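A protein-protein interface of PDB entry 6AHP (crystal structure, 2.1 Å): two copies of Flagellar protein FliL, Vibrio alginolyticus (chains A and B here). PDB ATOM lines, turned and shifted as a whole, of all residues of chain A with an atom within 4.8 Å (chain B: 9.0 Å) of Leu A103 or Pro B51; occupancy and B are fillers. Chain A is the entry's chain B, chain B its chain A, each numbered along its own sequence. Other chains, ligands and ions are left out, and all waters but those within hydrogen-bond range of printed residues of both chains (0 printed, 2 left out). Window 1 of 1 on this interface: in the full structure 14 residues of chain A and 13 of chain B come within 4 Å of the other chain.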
ATOM      1  N   TYR A   9       3.636   9.510 -17.228  1.00  0.00           N
ATOM      2  CA  TYR A   9       2.189   9.354 -17.333  1.00  0.00           C
ATOM      3  C   TYR A   9       1.793   9.402 -18.812  1.00  0.00           C
ATOM      4  O   TYR A   9       2.241  10.288 -19.534  1.00  0.00           O
ATOM      5  CB  TYR A   9       1.482  10.461 -16.497  1.00  0.00           C
ATOM      6  CG  TYR A   9       1.951  10.368 -15.045  1.00  0.00           C
ATOM      7  CD1 TYR A   9       1.525   9.322 -14.243  1.00  0.00           C
ATOM      8  CD2 TYR A   9       2.893  11.251 -14.531  1.00  0.00           C
ATOM      9  CE1 TYR A   9       1.986   9.161 -12.943  1.00  0.00           C
ATOM     10  CE2 TYR A   9       3.370  11.112 -13.216  1.00  0.00           C
ATOM     11  CZ  TYR A   9       2.915  10.058 -12.425  1.00  0.00           C
ATOM     12  OH  TYR A   9       3.351   9.885 -11.115  1.00  0.00           O
ATOM     13  N   LYS A  32     -12.437   8.761 -16.549  1.00  0.00           N
ATOM     14  CA  LYS A  32     -11.245   9.295 -17.189  1.00  0.00           C
ATOM     15  C   LYS A  32     -10.006   8.619 -16.598  1.00  0.00           C
ATOM     16  O   LYS A  32      -9.834   8.589 -15.373  1.00  0.00           O
ATOM     17  CB  LYS A  32     -11.169  10.803 -16.986  1.00  0.00           C
ATOM     18  CG  LYS A  32      -9.985  11.451 -17.662  1.00  0.00           C
ATOM     19  CD  LYS A  32     -10.093  11.388 -19.177  1.00  0.00           C
ATOM     20  CE  LYS A  32      -8.781  11.802 -19.823  1.00  0.00           C
ATOM     21  NZ  LYS A  32      -7.608  11.209 -19.078  1.00  0.00           N
ATOM     22  N   ALA A  33      -9.141   8.083 -17.459  1.00  0.00           N
ATOM     23  CA  ALA A  33      -7.992   7.324 -16.988  1.00  0.00           C
ATOM     24  C   ALA A  33      -6.692   7.841 -17.592  1.00  0.00           C
ATOM     25  O   ALA A  33      -6.678   8.493 -18.635  1.00  0.00           O
ATOM     26  CB  ALA A  33      -8.147   5.829 -17.297  1.00  0.00           C
ATOM     27  N   GLN A  34      -5.589   7.539 -16.902  1.00  0.00           N
ATOM     28  CA  GLN A  34      -4.232   7.732 -17.403  1.00  0.00           C
ATOM     29  C   GLN A  34      -3.434   6.496 -17.017  1.00  0.00           C
ATOM     30  O   GLN A  34      -3.852   5.701 -16.167  1.00  0.00           O
ATOM     31  CB  GLN A  34      -3.568   9.023 -16.872  1.00  0.00           C
ATOM     32  CG  GLN A  34      -4.254  10.307 -17.365  1.00  0.00           C
ATOM     33  CD  GLN A  34      -3.411  11.560 -17.243  1.00  0.00           C
ATOM     34  OE1 GLN A  34      -2.235  11.588 -17.620  1.00  0.00           O
ATOM     35  NE2 GLN A  34      -4.021  12.626 -16.722  1.00  0.00           N
ATOM     36  N   MET A  36       0.239   5.016 -15.660  1.00  0.00           N
ATOM     37  CA  MET A  36       1.509   5.271 -14.999  1.00  0.00           C
ATOM     38  C   MET A  36       2.522   4.233 -15.456  1.00  0.00           C
ATOM     39  O   MET A  36       2.277   3.034 -15.326  1.00  0.00           O
ATOM     40  CB  MET A  36       1.336   5.200 -13.472  1.00  0.00           C
ATOM     41  CG  MET A  36       2.630   5.391 -12.698  1.00  0.00           C
ATOM     42  SD  MET A  36       2.199   5.475 -10.902  1.00  0.00           S
ATOM     43  CE  MET A  36       3.581   6.428 -10.299  1.00  0.00           C
ATOM     44  N   LYS A 101       0.447   0.906 -13.268  1.00  0.00           N
ATOM     45  CA  LYS A 101      -0.966   0.754 -12.939  1.00  0.00           C
ATOM     46  C   LYS A 101      -1.745   1.793 -13.722  1.00  0.00           C
ATOM     47  O   LYS A 101      -1.164   2.734 -14.262  1.00  0.00           O
ATOM     48  CB  LYS A 101      -1.220   0.925 -11.436  1.00  0.00           C
ATOM     49  CG  LYS A 101      -0.718   2.262 -10.916  1.00  0.00           C
ATOM     50  CD  LYS A 101      -0.955   2.353  -9.411  1.00  0.00           C
ATOM     51  CE  LYS A 101      -0.270   3.563  -8.809  1.00  0.00           C
ATOM     52  NZ  LYS A 101       1.199   3.413  -8.928  1.00  0.00           N
ATOM     53  N   VAL A 102      -3.078   1.587 -13.790  1.00  0.00           N
ATOM     54  CA  VAL A 102      -4.041   2.564 -14.295  1.00  0.00           C
ATOM     55  C   VAL A 102      -4.387   3.550 -13.186  1.00  0.00           C
ATOM     56  O   VAL A 102      -4.623   3.155 -12.038  1.00  0.00           O
ATOM     57  CB  VAL A 102      -5.335   1.867 -14.777  1.00  0.00           C
ATOM     58  CG1 VAL A 102      -6.223   2.832 -15.572  1.00  0.00           C
ATOM     59  CG2 VAL A 102      -5.024   0.610 -15.560  1.00  0.00           C
ATOM     60  N   LEU A 103      -4.448   4.826 -13.540  1.00  0.00           N
ATOM     61  CA  LEU A 103      -4.878   5.901 -12.659  1.00  0.00           C
ATOM     62  C   LEU A 103      -6.247   6.380 -13.112  1.00  0.00           C
ATOM     63  O   LEU A 103      -6.500   6.506 -14.311  1.00  0.00           O
ATOM     64  CB  LEU A 103      -3.904   7.078 -12.690  1.00  0.00           C
ATOM     65  CG  LEU A 103      -2.438   6.780 -12.395  1.00  0.00           C
ATOM     66  CD1 LEU A 103      -1.593   8.010 -12.690  1.00  0.00           C
ATOM     67  CD2 LEU A 103      -2.257   6.245 -10.977  1.00  0.00           C
ATOM     68  N   PHE A 104      -7.132   6.630 -12.161  1.00  0.00           N
ATOM     69  CA  PHE A 104      -8.466   7.125 -12.470  1.00  0.00           C
ATOM     70  C   PHE A 104      -8.580   8.529 -11.923  1.00  0.00           C
ATOM     71  O   PHE A 104      -8.408   8.734 -10.723  1.00  0.00           O
ATOM     72  CB  PHE A 104      -9.514   6.184 -11.889  1.00  0.00           C
ATOM     73  CG  PHE A 104      -9.391   4.811 -12.439  1.00  0.00           C
ATOM     74  CD1 PHE A 104      -9.911   4.517 -13.674  1.00  0.00           C
ATOM     75  CD2 PHE A 104      -8.655   3.849 -11.787  1.00  0.00           C
ATOM     76  CE1 PHE A 104      -9.784   3.267 -14.218  1.00  0.00           C
ATOM     77  CE2 PHE A 104      -8.512   2.590 -12.327  1.00  0.00           C
ATOM     78  CZ  PHE A 104      -9.091   2.302 -13.544  1.00  0.00           C
ATOM     79  N   THR A 105      -8.752   9.478 -12.806  1.00  0.00           N
ATOM     80  CA  THR A 105      -8.861  10.856 -12.429  1.00  0.00           C
ATOM     81  C   THR A 105     -10.259  11.429 -12.314  1.00  0.00           C
ATOM     82  O   THR A 105     -10.405  12.440 -11.745  1.00  0.00           O
ATOM     83  CB  THR A 105      -8.039  11.792 -13.315  1.00  0.00           C
ATOM     84  OG1 THR A 105      -8.542  11.775 -14.624  1.00  0.00           O
ATOM     85  CG2 THR A 105      -6.599  11.419 -13.320  1.00  0.00           C
ATOM     86  N   LEU B  12      -5.090  22.884  -8.784  1.00  0.00           N
ATOM     87  CA  LEU B  12      -5.662  21.717  -9.435  1.00  0.00           C
ATOM     88  C   LEU B  12      -6.945  22.185 -10.105  1.00  0.00           C
ATOM     89  O   LEU B  12      -7.993  22.267  -9.442  1.00  0.00           O
ATOM     90  CB  LEU B  12      -5.947  20.609  -8.420  1.00  0.00           C
ATOM     91  CG  LEU B  12      -4.722  19.897  -7.855  1.00  0.00           C
ATOM     92  CD1 LEU B  12      -5.176  18.713  -7.082  1.00  0.00           C
ATOM     93  CD2 LEU B  12      -3.779  19.441  -8.975  1.00  0.00           C
ATOM     94  N   PHE B  16     -13.214  18.182  -8.073  1.00  0.00           N
ATOM     95  CA  PHE B  16     -13.544  16.777  -7.873  1.00  0.00           C
ATOM     96  C   PHE B  16     -15.044  16.634  -7.649  1.00  0.00           C
ATOM     97  O   PHE B  16     -15.611  17.259  -6.738  1.00  0.00           O
ATOM     98  CB  PHE B  16     -12.748  16.195  -6.706  1.00  0.00           C
ATOM     99  CG  PHE B  16     -11.287  16.183  -6.971  1.00  0.00           C
ATOM    100  CD1 PHE B  16     -10.694  15.092  -7.575  1.00  0.00           C
ATOM    101  CD2 PHE B  16     -10.523  17.309  -6.717  1.00  0.00           C
ATOM    102  CE1 PHE B  16      -9.326  15.098  -7.872  1.00  0.00           C
ATOM    103  CE2 PHE B  16      -9.166  17.337  -7.011  1.00  0.00           C
ATOM    104  CZ  PHE B  16      -8.562  16.225  -7.590  1.00  0.00           C
ATOM    105  N   LEU B  35      -2.760  22.523  -4.040  1.00  0.00           N
ATOM    106  CA  LEU B  35      -1.659  21.959  -3.273  1.00  0.00           C
ATOM    107  C   LEU B  35      -0.777  23.078  -2.731  1.00  0.00           C
ATOM    108  O   LEU B  35      -0.370  23.973  -3.480  1.00  0.00           O
ATOM    109  CB  LEU B  35      -0.815  21.000  -4.131  1.00  0.00           C
ATOM    110  CG  LEU B  35      -1.658  19.982  -4.917  1.00  0.00           C
ATOM    111  CD1 LEU B  35      -0.824  19.338  -6.003  1.00  0.00           C
ATOM    112  CD2 LEU B  35      -2.291  18.928  -3.944  1.00  0.00           C
ATOM    113  N   LEU B  45       7.833  19.065  -9.123  1.00  0.00           N
ATOM    114  CA  LEU B  45       7.385  17.691  -8.886  1.00  0.00           C
ATOM    115  C   LEU B  45       5.868  17.590  -8.773  1.00  0.00           C
ATOM    116  O   LEU B  45       5.262  16.663  -9.322  1.00  0.00           O
ATOM    117  CB  LEU B  45       8.028  17.134  -7.625  1.00  0.00           C
ATOM    118  CG  LEU B  45       9.515  16.815  -7.789  1.00  0.00           C
ATOM    119  CD1 LEU B  45      10.122  16.441  -6.455  1.00  0.00           C
ATOM    120  CD2 LEU B  45       9.680  15.675  -8.837  1.00  0.00           C
ATOM    121  N   ALA B  46       5.236  18.499  -8.016  1.00  0.00           N
ATOM    122  CA  ALA B  46       3.781  18.441  -7.859  1.00  0.00           C
ATOM    123  C   ALA B  46       3.078  18.601  -9.199  1.00  0.00           C
ATOM    124  O   ALA B  46       2.048  17.959  -9.457  1.00  0.00           O
ATOM    125  CB  ALA B  46       3.309  19.532  -6.885  1.00  0.00           C
ATOM    126  N   ARG B  47       3.616  19.459 -10.068  1.00  0.00           N
ATOM    127  CA  ARG B  47       3.009  19.626 -11.386  1.00  0.00           C
ATOM    128  C   ARG B  47       3.258  18.399 -12.271  1.00  0.00           C
ATOM    129  O   ARG B  47       2.355  17.953 -12.974  1.00  0.00           O
ATOM    130  CB  ARG B  47       3.540  20.886 -12.074  1.00  0.00           C
ATOM    131  CG  ARG B  47       3.365  22.148 -11.268  1.00  0.00           C
ATOM    132  CD  ARG B  47       3.766  23.365 -12.099  1.00  0.00           C
ATOM    133  NE  ARG B  47       3.564  24.611 -11.379  1.00  0.00           N
ATOM    134  CZ  ARG B  47       2.392  25.225 -11.278  1.00  0.00           C
ATOM    135  NH1 ARG B  47       1.315  24.700 -11.855  1.00  0.00           N
ATOM    136  NH2 ARG B  47       2.293  26.360 -10.599  1.00  0.00           N
ATOM    137  N   TYR B  48       4.467  17.835 -12.241  1.00  0.00           N
ATOM    138  CA  TYR B  48       4.755  16.705 -13.122  1.00  0.00           C
ATOM    139  C   TYR B  48       3.926  15.473 -12.745  1.00  0.00           C
ATOM    140  O   TYR B  48       3.444  14.742 -13.622  1.00  0.00           O
ATOM    141  CB  TYR B  48       6.252  16.400 -13.080  1.00  0.00           C
ATOM    142  CG  TYR B  48       6.674  15.217 -13.953  1.00  0.00           C
ATOM    143  CD1 TYR B  48       6.966  15.388 -15.321  1.00  0.00           C
ATOM    144  CD2 TYR B  48       6.794  13.955 -13.420  1.00  0.00           C
ATOM    145  CE1 TYR B  48       7.336  14.309 -16.117  1.00  0.00           C
ATOM    146  CE2 TYR B  48       7.177  12.864 -14.210  1.00  0.00           C
ATOM    147  CZ  TYR B  48       7.445  13.050 -15.552  1.00  0.00           C
ATOM    148  OH  TYR B  48       7.816  11.969 -16.316  1.00  0.00           O
ATOM    149  N   HIS B  49       3.752  15.227 -11.442  1.00  0.00           N
ATOM    150  CA  HIS B  49       3.031  14.067 -10.936  1.00  0.00           C
ATOM    151  C   HIS B  49       1.551  14.326 -10.711  1.00  0.00           C
ATOM    152  O   HIS B  49       0.898  13.554  -9.996  1.00  0.00           O
ATOM    153  CB  HIS B  49       3.699  13.585  -9.651  1.00  0.00           C
ATOM    154  CG  HIS B  49       5.049  13.003  -9.901  1.00  0.00           C
ATOM    155  ND1 HIS B  49       5.217  11.747 -10.443  1.00  0.00           N
ATOM    156  CD2 HIS B  49       6.290  13.531  -9.786  1.00  0.00           C
ATOM    157  CE1 HIS B  49       6.508  11.505 -10.599  1.00  0.00           C
ATOM    158  NE2 HIS B  49       7.179  12.568 -10.206  1.00  0.00           N
ATOM    159  N   SER B  50       1.015  15.397 -11.296  1.00  0.00           N
ATOM    160  CA  SER B  50      -0.412  15.702 -11.183  1.00  0.00           C
ATOM    161  C   SER B  50      -1.357  14.542 -11.483  1.00  0.00           C
ATOM    162  O   SER B  50      -2.389  14.440 -10.798  1.00  0.00           O
ATOM    163  CB  SER B  50      -0.763  16.878 -12.105  1.00  0.00           C
ATOM    164  OG  SER B  50      -0.609  18.074 -11.387  1.00  0.00           O
ATOM    165  N   PRO B  51      -1.114  13.678 -12.482  1.00  0.00           N
ATOM    166  CA  PRO B  51      -2.034  12.543 -12.667  1.00  0.00           C
ATOM    167  C   PRO B  51      -2.103  11.642 -11.452  1.00  0.00           C
ATOM    168  O   PRO B  51      -3.198  11.209 -11.054  1.00  0.00           O
ATOM    169  CB  PRO B  51      -1.451  11.814 -13.885  1.00  0.00           C
ATOM    170  CG  PRO B  51      -0.686  12.904 -14.626  1.00  0.00           C
ATOM    171  CD  PRO B  51      -0.071  13.709 -13.525  1.00  0.00           C
ATOM    172  N   LEU B  52      -0.954  11.374 -10.828  1.00  0.00           N
ATOM    173  CA  LEU B  52      -0.954  10.530  -9.637  1.00  0.00           C
ATOM    174  C   LEU B  52      -1.661  11.236  -8.477  1.00  0.00           C
ATOM    175  O   LEU B  52      -2.454  10.624  -7.757  1.00  0.00           O
ATOM    176  CB  LEU B  52       0.488  10.181  -9.277  1.00  0.00           C
ATOM    177  CG  LEU B  52       0.707   9.376  -8.010  1.00  0.00           C
ATOM    178  CD1 LEU B  52       0.093   7.992  -8.260  1.00  0.00           C
ATOM    179  CD2 LEU B  52       2.164   9.241  -7.679  1.00  0.00           C
ATOM    180  N   ILE B  53      -1.420  12.543  -8.330  1.00  0.00           N
ATOM    181  CA  ILE B  53      -2.025  13.300  -7.242  1.00  0.00           C
ATOM    182  C   ILE B  53      -3.546  13.332  -7.399  1.00  0.00           C
ATOM    183  O   ILE B  53      -4.285  13.082  -6.452  1.00  0.00           O
ATOM    184  CB  ILE B  53      -1.417  14.715  -7.176  1.00  0.00           C
ATOM    185  CG1 ILE B  53       0.035  14.616  -6.671  1.00  0.00           C
ATOM    186  CG2 ILE B  53      -2.255  15.633  -6.252  1.00  0.00           C
ATOM    187  CD1 ILE B  53       0.894  15.872  -6.861  1.00  0.00           C
ATOM    188  N   GLU B  54      -4.030  13.625  -8.607  1.00  0.00           N
ATOM    189  CA  GLU B  54      -5.474  13.679  -8.827  1.00  0.00           C
ATOM    190  C   GLU B  54      -6.123  12.335  -8.588  1.00  0.00           C
ATOM    191  O   GLU B  54      -7.259  12.262  -8.104  1.00  0.00           O
ATOM    192  CB  GLU B  54      -5.782  14.147 -10.248  1.00  0.00           C
ATOM    193  CG  GLU B  54      -5.401  15.568 -10.542  1.00  0.00           C
ATOM    194  CD  GLU B  54      -5.346  15.800 -12.044  1.00  0.00           C
ATOM    195  OE1 GLU B  54      -6.085  15.105 -12.777  1.00  0.00           O
ATOM    196  OE2 GLU B  54      -4.544  16.637 -12.503  1.00  0.00           O
ATOM    197  N   SER B  55      -5.420  11.259  -8.934  1.00  0.00           N
ATOM    198  CA  SER B  55      -5.954   9.920  -8.745  1.00  0.00           C
ATOM    199  C   SER B  55      -5.996   9.540  -7.269  1.00  0.00           C
ATOM    200  O   SER B  55      -6.922   8.852  -6.823  1.00  0.00           O
ATOM    201  CB  SER B  55      -5.106   8.926  -9.537  1.00  0.00           C
ATOM    202  OG  SER B  55      -5.899   7.802  -9.832  1.00  0.00           O
ATOM    203  N   SER B  56      -4.975   9.946  -6.507  1.00  0.00           N
ATOM    204  CA  SER B  56      -4.983   9.740  -5.065  1.00  0.00           C
ATOM    205  C   SER B  56      -6.159  10.459  -4.414  1.00  0.00           C
ATOM    206  O   SER B  56      -6.844   9.897  -3.559  1.00  0.00           O
ATOM    207  CB  SER B  56      -3.671  10.237  -4.464  1.00  0.00           C
ATOM    208  OG  SER B  56      -3.711  10.241  -3.053  1.00  0.00           O
ATOM    209  N   LEU B  57      -6.374  11.726  -4.785  1.00  0.00           N
ATOM    210  CA  LEU B  57      -7.487  12.499  -4.241  1.00  0.00           C
ATOM    211  C   LEU B  57      -8.829  11.815  -4.522  1.00  0.00           C
ATOM    212  O   LEU B  57      -9.668  11.675  -3.624  1.00  0.00           O
ATOM    213  CB  LEU B  57      -7.463  13.915  -4.826  1.00  0.00           C
ATOM    214  CG  LEU B  57      -6.462  14.859  -4.114  1.00  0.00           C
ATOM    215  CD1 LEU B  57      -6.234  16.178  -4.843  1.00  0.00           C
ATOM    216  CD2 LEU B  57      -6.831  15.093  -2.641  1.00  0.00           C
ATOM    217  N   LEU B  58      -9.065  11.415  -5.776  1.00  0.00           N
ATOM    218  CA  LEU B  58     -10.313  10.731  -6.112  1.00  0.00           C
ATOM    219  C   LEU B  58     -10.463   9.436  -5.321  1.00  0.00           C
ATOM    220  O   LEU B  58     -11.565   9.118  -4.862  1.00  0.00           O
ATOM    221  CB  LEU B  58     -10.394  10.461  -7.617  1.00  0.00           C
ATOM    222  CG  LEU B  58     -11.782  10.156  -8.200  1.00  0.00           C
ATOM    223  CD1 LEU B  58     -12.843  11.253  -7.858  1.00  0.00           C
ATOM    224  CD2 LEU B  58     -11.691   9.957  -9.715  1.00  0.00           C
ATOM    225  N   SER B  59      -9.362   8.692  -5.121  1.00  0.00           N
ATOM    226  CA  SER B  59      -9.417   7.493  -4.287  1.00  0.00           C
ATOM    227  C   SER B  59      -9.809   7.830  -2.861  1.00  0.00           C
ATOM    228  O   SER B  59     -10.597   7.107  -2.236  1.00  0.00           O
ATOM    229  CB  SER B  59      -8.074   6.770  -4.283  1.00  0.00           C
ATOM    230  OG  SER B  59      -7.809   6.153  -5.523  1.00  0.00           O
ATOM    231  N   ILE B  86      -1.712  11.426  -0.562  1.00  0.00           N
ATOM    232  CA  ILE B  86      -0.845  11.979  -1.615  1.00  0.00           C
ATOM    233  C   ILE B  86       0.623  11.803  -1.244  1.00  0.00           C
ATOM    234  O   ILE B  86       1.455  11.403  -2.066  1.00  0.00           O
ATOM    235  CB  ILE B  86      -1.161  13.469  -1.868  1.00  0.00           C
ATOM    236  CG1 ILE B  86      -2.509  13.646  -2.553  1.00  0.00           C
ATOM    237  CG2 ILE B  86      -0.032  14.141  -2.714  1.00  0.00           C
ATOM    238  CD1 ILE B  86      -3.104  15.062  -2.385  1.00  0.00           C
ATOM    239  N   ALA B  89       1.576   8.186  -1.727  1.00  0.00           N
ATOM    240  CA  ALA B  89       1.732   7.899  -3.161  1.00  0.00           C
ATOM    241  C   ALA B  89       3.033   8.463  -3.736  1.00  0.00           C
ATOM    242  O   ALA B  89       3.713   7.806  -4.537  1.00  0.00           O
ATOM    243  CB  ALA B  89       0.552   8.457  -3.962  1.00  0.00           C
ATOM    244  N   LEU B  90       3.370   9.691  -3.395  1.00  0.00           N
ATOM    245  CA  LEU B  90       4.584  10.259  -3.977  1.00  0.00           C
ATOM    246  C   LEU B  90       5.838   9.685  -3.319  1.00  0.00           C
ATOM    247  O   LEU B  90       6.864   9.515  -3.992  1.00  0.00           O
ATOM    248  CB  LEU B  90       4.552  11.784  -3.858  1.00  0.00           C
ATOM    249  CG  LEU B  90       3.418  12.415  -4.688  1.00  0.00           C
ATOM    250  CD1 LEU B  90       3.212  13.835  -4.290  1.00  0.00           C
ATOM    251  CD2 LEU B  90       3.754  12.352  -6.158  1.00  0.00           C
ATOM    252  N   ALA B  93       6.447   6.695  -5.080  1.00  0.00           N
ATOM    253  CA  ALA B  93       6.822   6.832  -6.479  1.00  0.00           C
ATOM    254  C   ALA B  93       8.197   7.475  -6.674  1.00  0.00           C
ATOM    255  O   ALA B  93       8.967   7.015  -7.520  1.00  0.00           O
ATOM    256  CB  ALA B  93       5.758   7.622  -7.232  1.00  0.00           C
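The backbone carbonyl oxygen of Phe A104 sits at hydrogen-bond distance from the side-chain hydroxyl of Ser B55, 2.8 Å away. A ring nitrogen (ND1) of His B49 sits at hydrogen-bond distance from the side-chain hydroxyl of Tyr A9, 2.7 Å away.
The backbone carbonyl oxygen of Ser B55 sits at hydrogen-bond distance from the side-chain hydroxyl of Ser B59 (3.1 Å). O of Gln A34 lies within hydrogen-bond range of N of Leu A103, 2.8 Å away. The backbone carbonyl oxygen (O) of Lys A32 lies within hydrogen-bond range of the backbone NH (N) of Thr A105 (2.9 Å). N of Met A36 lies within hydrogen-bond range of O of Lys A101, at 3.0 Å.
Among the printed residues, pairs that only touch across the chains: Thr A105 with Leu B58, Tyr A9 with Leu B52, Leu A103 with Ser B55, Gln A34 with Pro B51, Phe A104 with Leu B58, Tyr A9 with Tyr B48, Tyr A9 with Pro B51, Thr A105 with Glu B54, Leu A103 with Pro B51, Leu A103 with Leu B52 and Met A36 with Ala B93.
Lys A32 touches none of the printed residues of chain B. Gln A34 touches just one residue of chain B: Pro B51. Val A102 touches none of the printed residues of chain B. Of the printed residues of chain B, Leu A103 touches Pro B51, Leu B52 and Ser B55. Leu B35 touches none of the printed residues of chain A. Of the printed residues of chain A, His B49 touches Tyr A9 (2.7 Å). Pro B51 touches just these residues of chain A: Tyr A9, Gln A34 and Leu A103. Printed residues of chain A within 4 Å of Leu B52: Tyr A9 and Leu A103. Printed residues of chain A within 4 Å of Ser B55: Leu A103 and Phe A104. The nearest residue of chain B that does not touch Leu A103 is Ile B53 (6.3 Å). The nearest residue of chain A that does not touch Pro B51 is Thr A105 (4.1 Å).
Of the 22 printed residues of chain B, 8 touch a printed residue of chain A. Printed residues of chain B that touch a printed residue of chain A: Tyr B48, His B49, Pro B51, Leu B52, Glu B54, Ser B55, Leu B58 and Ala B93. Along chain B the printed residues that touch a printed residue of chain A span positions 48 to 93. Of the 10 printed residues of chain A, 6 touch a printed residue of chain B. Printed residues of chain A that touch a printed residue of chain B: Tyr A9, Gln A34, Met A36, Leu A103, Phe A104 and Thr A105. Hydrophobic or aromatic side chains of chain A within 4 Å of the printed part of chain B: Tyr A9, Met A36 and Leu A103. Among the printed residues, no Asp or Glu carboxylate lies within 4 Å of a Lys or Arg side-chain nitrogen of the other chain.
No position is printed for both chains. Of the 13 pairs that touch across the chains among the printed residues, none has its exchanged pair printed and touching as well.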
